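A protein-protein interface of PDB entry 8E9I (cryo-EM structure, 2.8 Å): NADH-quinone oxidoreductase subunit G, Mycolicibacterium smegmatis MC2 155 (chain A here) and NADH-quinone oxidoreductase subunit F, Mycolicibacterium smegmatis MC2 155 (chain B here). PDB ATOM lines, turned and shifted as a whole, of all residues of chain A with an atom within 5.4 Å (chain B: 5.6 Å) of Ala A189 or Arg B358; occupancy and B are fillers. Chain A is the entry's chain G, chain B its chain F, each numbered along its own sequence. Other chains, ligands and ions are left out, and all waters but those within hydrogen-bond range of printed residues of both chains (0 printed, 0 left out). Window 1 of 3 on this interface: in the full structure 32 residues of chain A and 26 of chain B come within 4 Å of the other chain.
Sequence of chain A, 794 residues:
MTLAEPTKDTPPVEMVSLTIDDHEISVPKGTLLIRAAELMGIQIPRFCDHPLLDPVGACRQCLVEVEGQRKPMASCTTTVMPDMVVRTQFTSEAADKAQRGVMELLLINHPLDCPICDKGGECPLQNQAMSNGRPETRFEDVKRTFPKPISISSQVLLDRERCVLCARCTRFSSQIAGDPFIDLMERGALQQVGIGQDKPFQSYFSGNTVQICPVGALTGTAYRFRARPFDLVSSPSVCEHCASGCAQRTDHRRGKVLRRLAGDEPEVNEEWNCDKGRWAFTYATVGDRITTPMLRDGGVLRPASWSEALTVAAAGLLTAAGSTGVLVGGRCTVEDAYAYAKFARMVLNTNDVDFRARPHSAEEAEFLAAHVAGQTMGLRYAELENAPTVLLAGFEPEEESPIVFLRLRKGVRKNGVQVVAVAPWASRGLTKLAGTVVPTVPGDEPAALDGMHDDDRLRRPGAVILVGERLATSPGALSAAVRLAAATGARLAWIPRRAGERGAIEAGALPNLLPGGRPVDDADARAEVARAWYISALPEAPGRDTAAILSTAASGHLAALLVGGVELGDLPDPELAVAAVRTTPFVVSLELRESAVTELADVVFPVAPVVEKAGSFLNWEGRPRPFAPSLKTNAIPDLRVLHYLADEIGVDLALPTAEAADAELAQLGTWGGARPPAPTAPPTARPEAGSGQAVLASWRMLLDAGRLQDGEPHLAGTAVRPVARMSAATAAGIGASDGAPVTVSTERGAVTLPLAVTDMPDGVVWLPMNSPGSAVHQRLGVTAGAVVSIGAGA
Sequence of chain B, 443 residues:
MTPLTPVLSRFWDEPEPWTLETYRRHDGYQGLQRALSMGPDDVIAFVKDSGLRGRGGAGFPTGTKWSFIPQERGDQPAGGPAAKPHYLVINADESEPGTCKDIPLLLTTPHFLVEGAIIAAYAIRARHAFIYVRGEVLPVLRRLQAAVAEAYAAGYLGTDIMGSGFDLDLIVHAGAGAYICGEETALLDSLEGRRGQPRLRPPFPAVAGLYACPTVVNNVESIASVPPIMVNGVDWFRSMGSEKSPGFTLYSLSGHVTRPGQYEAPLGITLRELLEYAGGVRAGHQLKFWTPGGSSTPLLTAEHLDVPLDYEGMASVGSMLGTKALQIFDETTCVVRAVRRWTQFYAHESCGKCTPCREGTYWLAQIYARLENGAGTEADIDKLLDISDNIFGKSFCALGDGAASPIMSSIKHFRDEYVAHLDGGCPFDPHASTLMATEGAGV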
ATOM      1  N   CYS A  59     -30.847  -3.310 -21.764  1.00  0.00           N
ATOM      2  CA  CYS A  59     -30.800  -4.320 -22.807  1.00  0.00           C
ATOM      3  C   CYS A  59     -31.265  -3.806 -24.158  1.00  0.00           C
ATOM      4  O   CYS A  59     -30.973  -4.444 -25.173  1.00  0.00           O
ATOM      5  CB  CYS A  59     -31.639  -5.528 -22.399  1.00  0.00           C
ATOM      6  SG  CYS A  59     -33.399  -5.316 -22.642  1.00  0.00           S
ATOM      7  N   LEU A 106     -28.376 -10.452 -28.771  1.00  0.00           N
ATOM      8  CA  LEU A 106     -28.544 -11.039 -27.454  1.00  0.00           C
ATOM      9  C   LEU A 106     -28.264 -12.529 -27.471  1.00  0.00           C
ATOM     10  O   LEU A 106     -27.836 -13.086 -26.456  1.00  0.00           O
ATOM     11  CB  LEU A 106     -29.961 -10.760 -26.960  1.00  0.00           C
ATOM     12  CG  LEU A 106     -30.229 -10.684 -25.465  1.00  0.00           C
ATOM     13  CD1 LEU A 106     -29.489  -9.543 -24.823  1.00  0.00           C
ATOM     14  CD2 LEU A 106     -31.712 -10.502 -25.274  1.00  0.00           C
ATOM     15  N   ARG A 144     -18.672 -15.988 -26.788  1.00  0.00           N
ATOM     16  CA  ARG A 144     -18.027 -15.694 -25.518  1.00  0.00           C
ATOM     17  C   ARG A 144     -18.238 -16.862 -24.572  1.00  0.00           C
ATOM     18  O   ARG A 144     -19.269 -17.536 -24.617  1.00  0.00           O
ATOM     19  CB  ARG A 144     -18.602 -14.422 -24.901  1.00  0.00           C
ATOM     20  CG  ARG A 144     -18.061 -14.125 -23.515  1.00  0.00           C
ATOM     21  CD  ARG A 144     -18.615 -12.833 -22.972  1.00  0.00           C
ATOM     22  NE  ARG A 144     -20.046 -12.940 -22.712  1.00  0.00           N
ATOM     23  CZ  ARG A 144     -20.969 -12.096 -23.153  1.00  0.00           C
ATOM     24  NH1 ARG A 144     -20.656 -11.049 -23.901  1.00  0.00           N
ATOM     25  NH2 ARG A 144     -22.241 -12.304 -22.831  1.00  0.00           N
ATOM     26  N   PHE A 146     -17.512 -18.371 -20.425  1.00  0.00           N
ATOM     27  CA  PHE A 146     -17.099 -18.272 -19.039  1.00  0.00           C
ATOM     28  C   PHE A 146     -17.086 -19.662 -18.427  1.00  0.00           C
ATOM     29  O   PHE A 146     -17.859 -20.530 -18.842  1.00  0.00           O
ATOM     30  CB  PHE A 146     -18.047 -17.392 -18.216  1.00  0.00           C
ATOM     31  CG  PHE A 146     -18.011 -15.944 -18.574  1.00  0.00           C
ATOM     32  CD1 PHE A 146     -17.015 -15.126 -18.086  1.00  0.00           C
ATOM     33  CD2 PHE A 146     -18.998 -15.391 -19.362  1.00  0.00           C
ATOM     34  CE1 PHE A 146     -16.988 -13.791 -18.401  1.00  0.00           C
ATOM     35  CE2 PHE A 146     -18.980 -14.055 -19.677  1.00  0.00           C
ATOM     36  CZ  PHE A 146     -17.976 -13.253 -19.196  1.00  0.00           C
ATOM     37  N   VAL A 164     -27.724 -12.232 -19.717  1.00  0.00           N
ATOM     38  CA  VAL A 164     -27.943 -11.215 -20.736  1.00  0.00           C
ATOM     39  C   VAL A 164     -27.559  -9.852 -20.176  1.00  0.00           C
ATOM     40  O   VAL A 164     -27.817  -8.820 -20.800  1.00  0.00           O
ATOM     41  CB  VAL A 164     -29.403 -11.218 -21.224  1.00  0.00           C
ATOM     42  CG1 VAL A 164     -29.698 -12.501 -21.960  1.00  0.00           C
ATOM     43  CG2 VAL A 164     -30.365 -11.044 -20.064  1.00  0.00           C
ATOM     44  N   LEU A 165     -26.956  -9.839 -18.990  1.00  0.00           N
ATOM     45  CA  LEU A 165     -26.476  -8.605 -18.369  1.00  0.00           C
ATOM     46  C   LEU A 165     -27.567  -7.546 -18.323  1.00  0.00           C
ATOM     47  O   LEU A 165     -27.328  -6.372 -18.596  1.00  0.00           O
ATOM     48  CB  LEU A 165     -25.239  -8.073 -19.086  1.00  0.00           C
ATOM     49  CG  LEU A 165     -23.985  -8.912 -18.874  1.00  0.00           C
ATOM     50  CD1 LEU A 165     -23.018  -8.731 -20.025  1.00  0.00           C
ATOM     51  CD2 LEU A 165     -23.330  -8.542 -17.563  1.00  0.00           C
ATOM     52  N   ARG A 187     -15.723  -5.199 -17.784  1.00  0.00           N
ATOM     53  CA  ARG A 187     -16.153  -4.159 -18.703  1.00  0.00           C
ATOM     54  C   ARG A 187     -16.324  -4.741 -20.094  1.00  0.00           C
ATOM     55  O   ARG A 187     -15.784  -5.801 -20.410  1.00  0.00           O
ATOM     56  CB  ARG A 187     -15.142  -3.015 -18.735  1.00  0.00           C
ATOM     57  CG  ARG A 187     -15.537  -1.855 -19.608  1.00  0.00           C
ATOM     58  CD  ARG A 187     -14.807  -0.611 -19.189  1.00  0.00           C
ATOM     59  NE  ARG A 187     -13.376  -0.739 -19.433  1.00  0.00           N
ATOM     60  CZ  ARG A 187     -12.688  -0.048 -20.331  1.00  0.00           C
ATOM     61  NH1 ARG A 187     -13.259   0.876 -21.086  1.00  0.00           N
ATOM     62  NH2 ARG A 187     -11.388  -0.284 -20.470  1.00  0.00           N
ATOM     63  N   GLY A 188     -17.083  -4.030 -20.920  1.00  0.00           N
ATOM     64  CA  GLY A 188     -17.211  -4.421 -22.310  1.00  0.00           C
ATOM     65  C   GLY A 188     -17.888  -5.766 -22.441  1.00  0.00           C
ATOM     66  O   GLY A 188     -18.740  -6.143 -21.631  1.00  0.00           O
ATOM     67  N   ALA A 189     -17.496  -6.515 -23.469  1.00  0.00           N
ATOM     68  CA  ALA A 189     -18.091  -7.829 -23.682  1.00  0.00           C
ATOM     69  C   ALA A 189     -17.865  -8.741 -22.488  1.00  0.00           C
ATOM     70  O   ALA A 189     -18.606  -9.712 -22.301  1.00  0.00           O
ATOM     71  CB  ALA A 189     -17.518  -8.463 -24.946  1.00  0.00           C
ATOM     72  N   LEU A 190     -16.863  -8.444 -21.670  1.00  0.00           N
ATOM     73  CA  LEU A 190     -16.502  -9.280 -20.538  1.00  0.00           C
ATOM     74  C   LEU A 190     -17.316  -8.978 -19.289  1.00  0.00           C
ATOM     75  O   LEU A 190     -17.090  -9.612 -18.256  1.00  0.00           O
ATOM     76  CB  LEU A 190     -15.015  -9.109 -20.229  1.00  0.00           C
ATOM     77  CG  LEU A 190     -14.394 -10.136 -19.288  1.00  0.00           C
ATOM     78  CD1 LEU A 190     -14.550 -11.531 -19.852  1.00  0.00           C
ATOM     79  CD2 LEU A 190     -12.936  -9.815 -19.058  1.00  0.00           C
ATOM     80  N   GLN A 191     -18.248  -8.032 -19.349  1.00  0.00           N
ATOM     81  CA  GLN A 191     -19.005  -7.668 -18.161  1.00  0.00           C
ATOM     82  C   GLN A 191     -19.767  -8.873 -17.629  1.00  0.00           C
ATOM     83  O   GLN A 191     -20.295  -9.681 -18.394  1.00  0.00           O
ATOM     84  CB  GLN A 191     -19.969  -6.529 -18.473  1.00  0.00           C
ATOM     85  CG  GLN A 191     -20.585  -5.918 -17.243  1.00  0.00           C
ATOM     86  CD  GLN A 191     -21.437  -4.714 -17.555  1.00  0.00           C
ATOM     87  OE1 GLN A 191     -21.067  -3.584 -17.245  1.00  0.00           O
ATOM     88  NE2 GLN A 191     -22.587  -4.946 -18.166  1.00  0.00           N
ATOM     89  N   ALA B 347     -14.724  -2.388 -28.852  1.00  0.00           N
ATOM     90  CA  ALA B 347     -15.064  -3.550 -28.046  1.00  0.00           C
ATOM     91  C   ALA B 347     -14.354  -3.510 -26.705  1.00  0.00           C
ATOM     92  O   ALA B 347     -14.958  -3.811 -25.672  1.00  0.00           O
ATOM     93  CB  ALA B 347     -14.713  -4.834 -28.791  1.00  0.00           C
ATOM     94  N   SER B 350     -15.932  -0.523 -24.596  1.00  0.00           N
ATOM     95  CA  SER B 350     -17.357  -0.530 -24.307  1.00  0.00           C
ATOM     96  C   SER B 350     -17.590  -0.721 -22.820  1.00  0.00           C
ATOM     97  O   SER B 350     -16.884  -1.485 -22.162  1.00  0.00           O
ATOM     98  CB  SER B 350     -18.052  -1.647 -25.079  1.00  0.00           C
ATOM     99  OG  SER B 350     -18.166  -1.319 -26.446  1.00  0.00           O
ATOM    100  N   GLY B 352     -20.272  -2.056 -21.702  1.00  0.00           N
ATOM    101  CA  GLY B 352     -21.008  -3.294 -21.600  1.00  0.00           C
ATOM    102  C   GLY B 352     -22.449  -3.137 -21.179  1.00  0.00           C
ATOM    103  O   GLY B 352     -23.157  -4.143 -21.070  1.00  0.00           O
ATOM    104  N   LYS B 353     -22.913  -1.909 -20.959  1.00  0.00           N
ATOM    105  CA  LYS B 353     -24.216  -1.721 -20.340  1.00  0.00           C
ATOM    106  C   LYS B 353     -25.339  -2.269 -21.208  1.00  0.00           C
ATOM    107  O   LYS B 353     -26.214  -2.988 -20.715  1.00  0.00           O
ATOM    108  CB  LYS B 353     -24.442  -0.242 -20.049  1.00  0.00           C
ATOM    109  CG  LYS B 353     -25.811   0.068 -19.489  1.00  0.00           C
ATOM    110  CD  LYS B 353     -25.880   1.473 -18.954  1.00  0.00           C
ATOM    111  CE  LYS B 353     -27.243   1.762 -18.378  1.00  0.00           C
ATOM    112  NZ  LYS B 353     -27.171   2.738 -17.263  1.00  0.00           N
ATOM    113  N   CYS B 354     -25.335  -1.953 -22.499  1.00  0.00           N
ATOM    114  CA  CYS B 354     -26.469  -2.235 -23.368  1.00  0.00           C
ATOM    115  C   CYS B 354     -26.121  -3.318 -24.376  1.00  0.00           C
ATOM    116  O   CYS B 354     -24.988  -3.397 -24.854  1.00  0.00           O
ATOM    117  CB  CYS B 354     -26.933  -0.967 -24.089  1.00  0.00           C
ATOM    118  SG  CYS B 354     -25.791  -0.296 -25.294  1.00  0.00           S
ATOM    119  N   THR B 355     -27.112  -4.152 -24.691  1.00  0.00           N
ATOM    120  CA  THR B 355     -26.878  -5.278 -25.593  1.00  0.00           C
ATOM    121  C   THR B 355     -26.317  -4.842 -26.934  1.00  0.00           C
ATOM    122  O   THR B 355     -25.324  -5.439 -27.384  1.00  0.00           O
ATOM    123  CB  THR B 355     -28.172  -6.073 -25.789  1.00  0.00           C
ATOM    124  OG1 THR B 355     -28.690  -6.473 -24.519  1.00  0.00           O
ATOM    125  CG2 THR B 355     -27.916  -7.313 -26.630  1.00  0.00           C
ATOM    126  N   PRO B 356     -26.876  -3.842 -27.623  1.00  0.00           N
ATOM    127  CA  PRO B 356     -26.357  -3.531 -28.961  1.00  0.00           C
ATOM    128  C   PRO B 356     -24.859  -3.308 -28.984  1.00  0.00           C
ATOM    129  O   PRO B 356     -24.149  -4.057 -29.649  1.00  0.00           O
ATOM    130  CB  PRO B 356     -27.145  -2.275 -29.347  1.00  0.00           C
ATOM    131  CG  PRO B 356     -28.389  -2.376 -28.588  1.00  0.00           C
ATOM    132  CD  PRO B 356     -28.008  -2.972 -27.273  1.00  0.00           C
ATOM    133  N   CYS B 357     -24.336  -2.328 -28.254  1.00  0.00           N
ATOM    134  CA  CYS B 357     -22.900  -2.090 -28.320  1.00  0.00           C
ATOM    135  C   CYS B 357     -22.127  -3.293 -27.797  1.00  0.00           C
ATOM    136  O   CYS B 357     -21.284  -3.851 -28.506  1.00  0.00           O
ATOM    137  CB  CYS B 357     -22.547  -0.823 -27.543  1.00  0.00           C
ATOM    138  SG  CYS B 357     -20.795  -0.587 -27.176  1.00  0.00           S
ATOM    139  N   ARG B 358     -22.456  -3.752 -26.589  1.00  0.00           N
ATOM    140  CA  ARG B 358     -21.677  -4.803 -25.945  1.00  0.00           C
ATOM    141  C   ARG B 358     -21.509  -6.006 -26.862  1.00  0.00           C
ATOM    142  O   ARG B 358     -20.399  -6.511 -27.050  1.00  0.00           O
ATOM    143  CB  ARG B 358     -22.345  -5.229 -24.638  1.00  0.00           C
ATOM    144  CG  ARG B 358     -21.720  -6.468 -24.025  1.00  0.00           C
ATOM    145  CD  ARG B 358     -22.284  -6.811 -22.664  1.00  0.00           C
ATOM    146  NE  ARG B 358     -23.595  -6.227 -22.421  1.00  0.00           N
ATOM    147  CZ  ARG B 358     -24.745  -6.827 -22.692  1.00  0.00           C
ATOM    148  NH1 ARG B 358     -24.787  -8.017 -23.265  1.00  0.00           N
ATOM    149  NH2 ARG B 358     -25.881  -6.212 -22.390  1.00  0.00           N
ATOM    150  N   GLU B 359     -22.608  -6.480 -27.442  1.00  0.00           N
ATOM    151  CA  GLU B 359     -22.564  -7.689 -28.253  1.00  0.00           C
ATOM    152  C   GLU B 359     -22.140  -7.416 -29.691  1.00  0.00           C
ATOM    153  O   GLU B 359     -21.324  -8.161 -30.248  1.00  0.00           O
ATOM    154  CB  GLU B 359     -23.931  -8.370 -28.237  1.00  0.00           C
ATOM    155  N   GLY B 360     -22.687  -6.374 -30.314  1.00  0.00           N
ATOM    156  CA  GLY B 360     -22.387  -6.116 -31.706  1.00  0.00           C
ATOM    157  C   GLY B 360     -20.938  -5.748 -31.939  1.00  0.00           C
ATOM    158  O   GLY B 360     -20.361  -6.107 -32.961  1.00  0.00           O
ATOM    159  N   THR B 361     -20.333  -4.999 -31.016  1.00  0.00           N
ATOM    160  CA  THR B 361     -18.922  -4.679 -31.182  1.00  0.00           C
ATOM    161  C   THR B 361     -18.070  -5.930 -31.113  1.00  0.00           C
ATOM    162  O   THR B 361     -17.132  -6.086 -31.897  1.00  0.00           O
ATOM    163  CB  THR B 361     -18.473  -3.680 -30.123  1.00  0.00           C
ATOM    164  OG1 THR B 361     -18.778  -4.199 -28.823  1.00  0.00           O
ATOM    165  CG2 THR B 361     -19.167  -2.349 -30.323  1.00  0.00           C
ATOM    166  N   TYR B 362     -18.383  -6.832 -30.187  1.00  0.00           N
ATOM    167  CA  TYR B 362     -17.683  -8.110 -30.120  1.00  0.00           C
ATOM    168  C   TYR B 362     -17.820  -8.863 -31.436  1.00  0.00           C
ATOM    169  O   TYR B 362     -16.829  -9.341 -32.011  1.00  0.00           O
ATOM    170  CB  TYR B 362     -18.257  -8.914 -28.952  1.00  0.00           C
ATOM    171  CG  TYR B 362     -17.757 -10.328 -28.794  1.00  0.00           C
ATOM    172  CD1 TYR B 362     -18.264 -11.358 -29.573  1.00  0.00           C
ATOM    173  CD2 TYR B 362     -16.821 -10.645 -27.824  1.00  0.00           C
ATOM    174  CE1 TYR B 362     -17.821 -12.651 -29.415  1.00  0.00           C
ATOM    175  CE2 TYR B 362     -16.376 -11.935 -27.661  1.00  0.00           C
ATOM    176  CZ  TYR B 362     -16.883 -12.934 -28.459  1.00  0.00           C
ATOM    177  OH  TYR B 362     -16.442 -14.225 -28.299  1.00  0.00           O
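NE of Arg B358 sits at hydrogen-bond distance from O of Gly B352 (2.5 Å). The guanidinium group of Arg A144 is in hydrogen-bond range of the backbone carbonyl oxygen of Ala A189 (2.9 Å). The side-chain sulfur (SG) of Cys B357 sits close to the side-chain hydroxyl (OG) of Ser B350 (2.8 Å). The backbone carbonyl oxygen (O) of Arg B358 lies within hydrogen-bond range of the side-chain hydroxyl (OG1) of Thr B361, at 3.3 Å.
O of Gly B352 lies within hydrogen-bond range of NE2 of Gln A191 (3.1 Å). OH of Tyr B362 sits at hydrogen-bond distance from N of Arg A144 (3.2 Å). The backbone carbonyl oxygen (O) of Cys A59 sits at hydrogen-bond distance from the side-chain hydroxyl (OG1) of Thr B355. The backbone NH (N) of Gly A188 sits at hydrogen-bond distance from the backbone carbonyl oxygen (O) of Ser B350, at 2.8 Å.
Printed residues of chain B within 4 Å of Leu A106: Thr B355 (3.2 Å). Printed residues of chain B within 4 Å of Leu A165: Arg B358. Ala A189 touches just these residues of chain B: Arg B358 and Tyr B362. Of the printed residues of chain A, Thr B355 touches Cys A59 and Leu A106. Printed residues of chain A within 4 Å of Pro B356: Cys A59. Cys B357 touches none of the printed residues of chain A. Arg B358 touches four residues of chain A. Of the printed residues of chain A, Tyr B362 touches Arg A144 (3.2 Å) and Ala A189 (3.7 Å). The nearest residue of chain B that does not touch Ala A189 is Ala B347 (4.3 Å). The nearest residue of chain A that does not touch Arg B358 is Gln A191 (4.6 Å).
Hydrophobic or aromatic side chains of chain B within 4 Å of the printed part of chain A: Pro B356 and Tyr B362. Of the 11 printed residues of chain A, 9 touch a printed residue of chain B. Hydrophobic or aromatic side chains of chain A within 4 Å of the printed part of chain B: Leu A106, Leu A165 and Ala A189. Among the printed residues, no Asp or Glu carboxylate lies within 4 Å of a Lys or Arg side-chain nitrogen of the other chain.
Among the printed residues, pairs that only touch across the chains: Cys A59 with Pro B356 (3.9 Å), Leu A106 with Thr B355 (3.2 Å), Val A164 with Arg B358 (3.6 Å), Leu A165 with Arg B358 (3.3 Å), Arg A187 with Ser B350 (2.9 Å), Gly A188 with Gly B352 (3.6 Å), Gly A188 with Arg B358 (3.8 Å), Ala A189 with Arg B358 (3.9 Å) and Ala A189 with Tyr B362 (3.7 Å).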
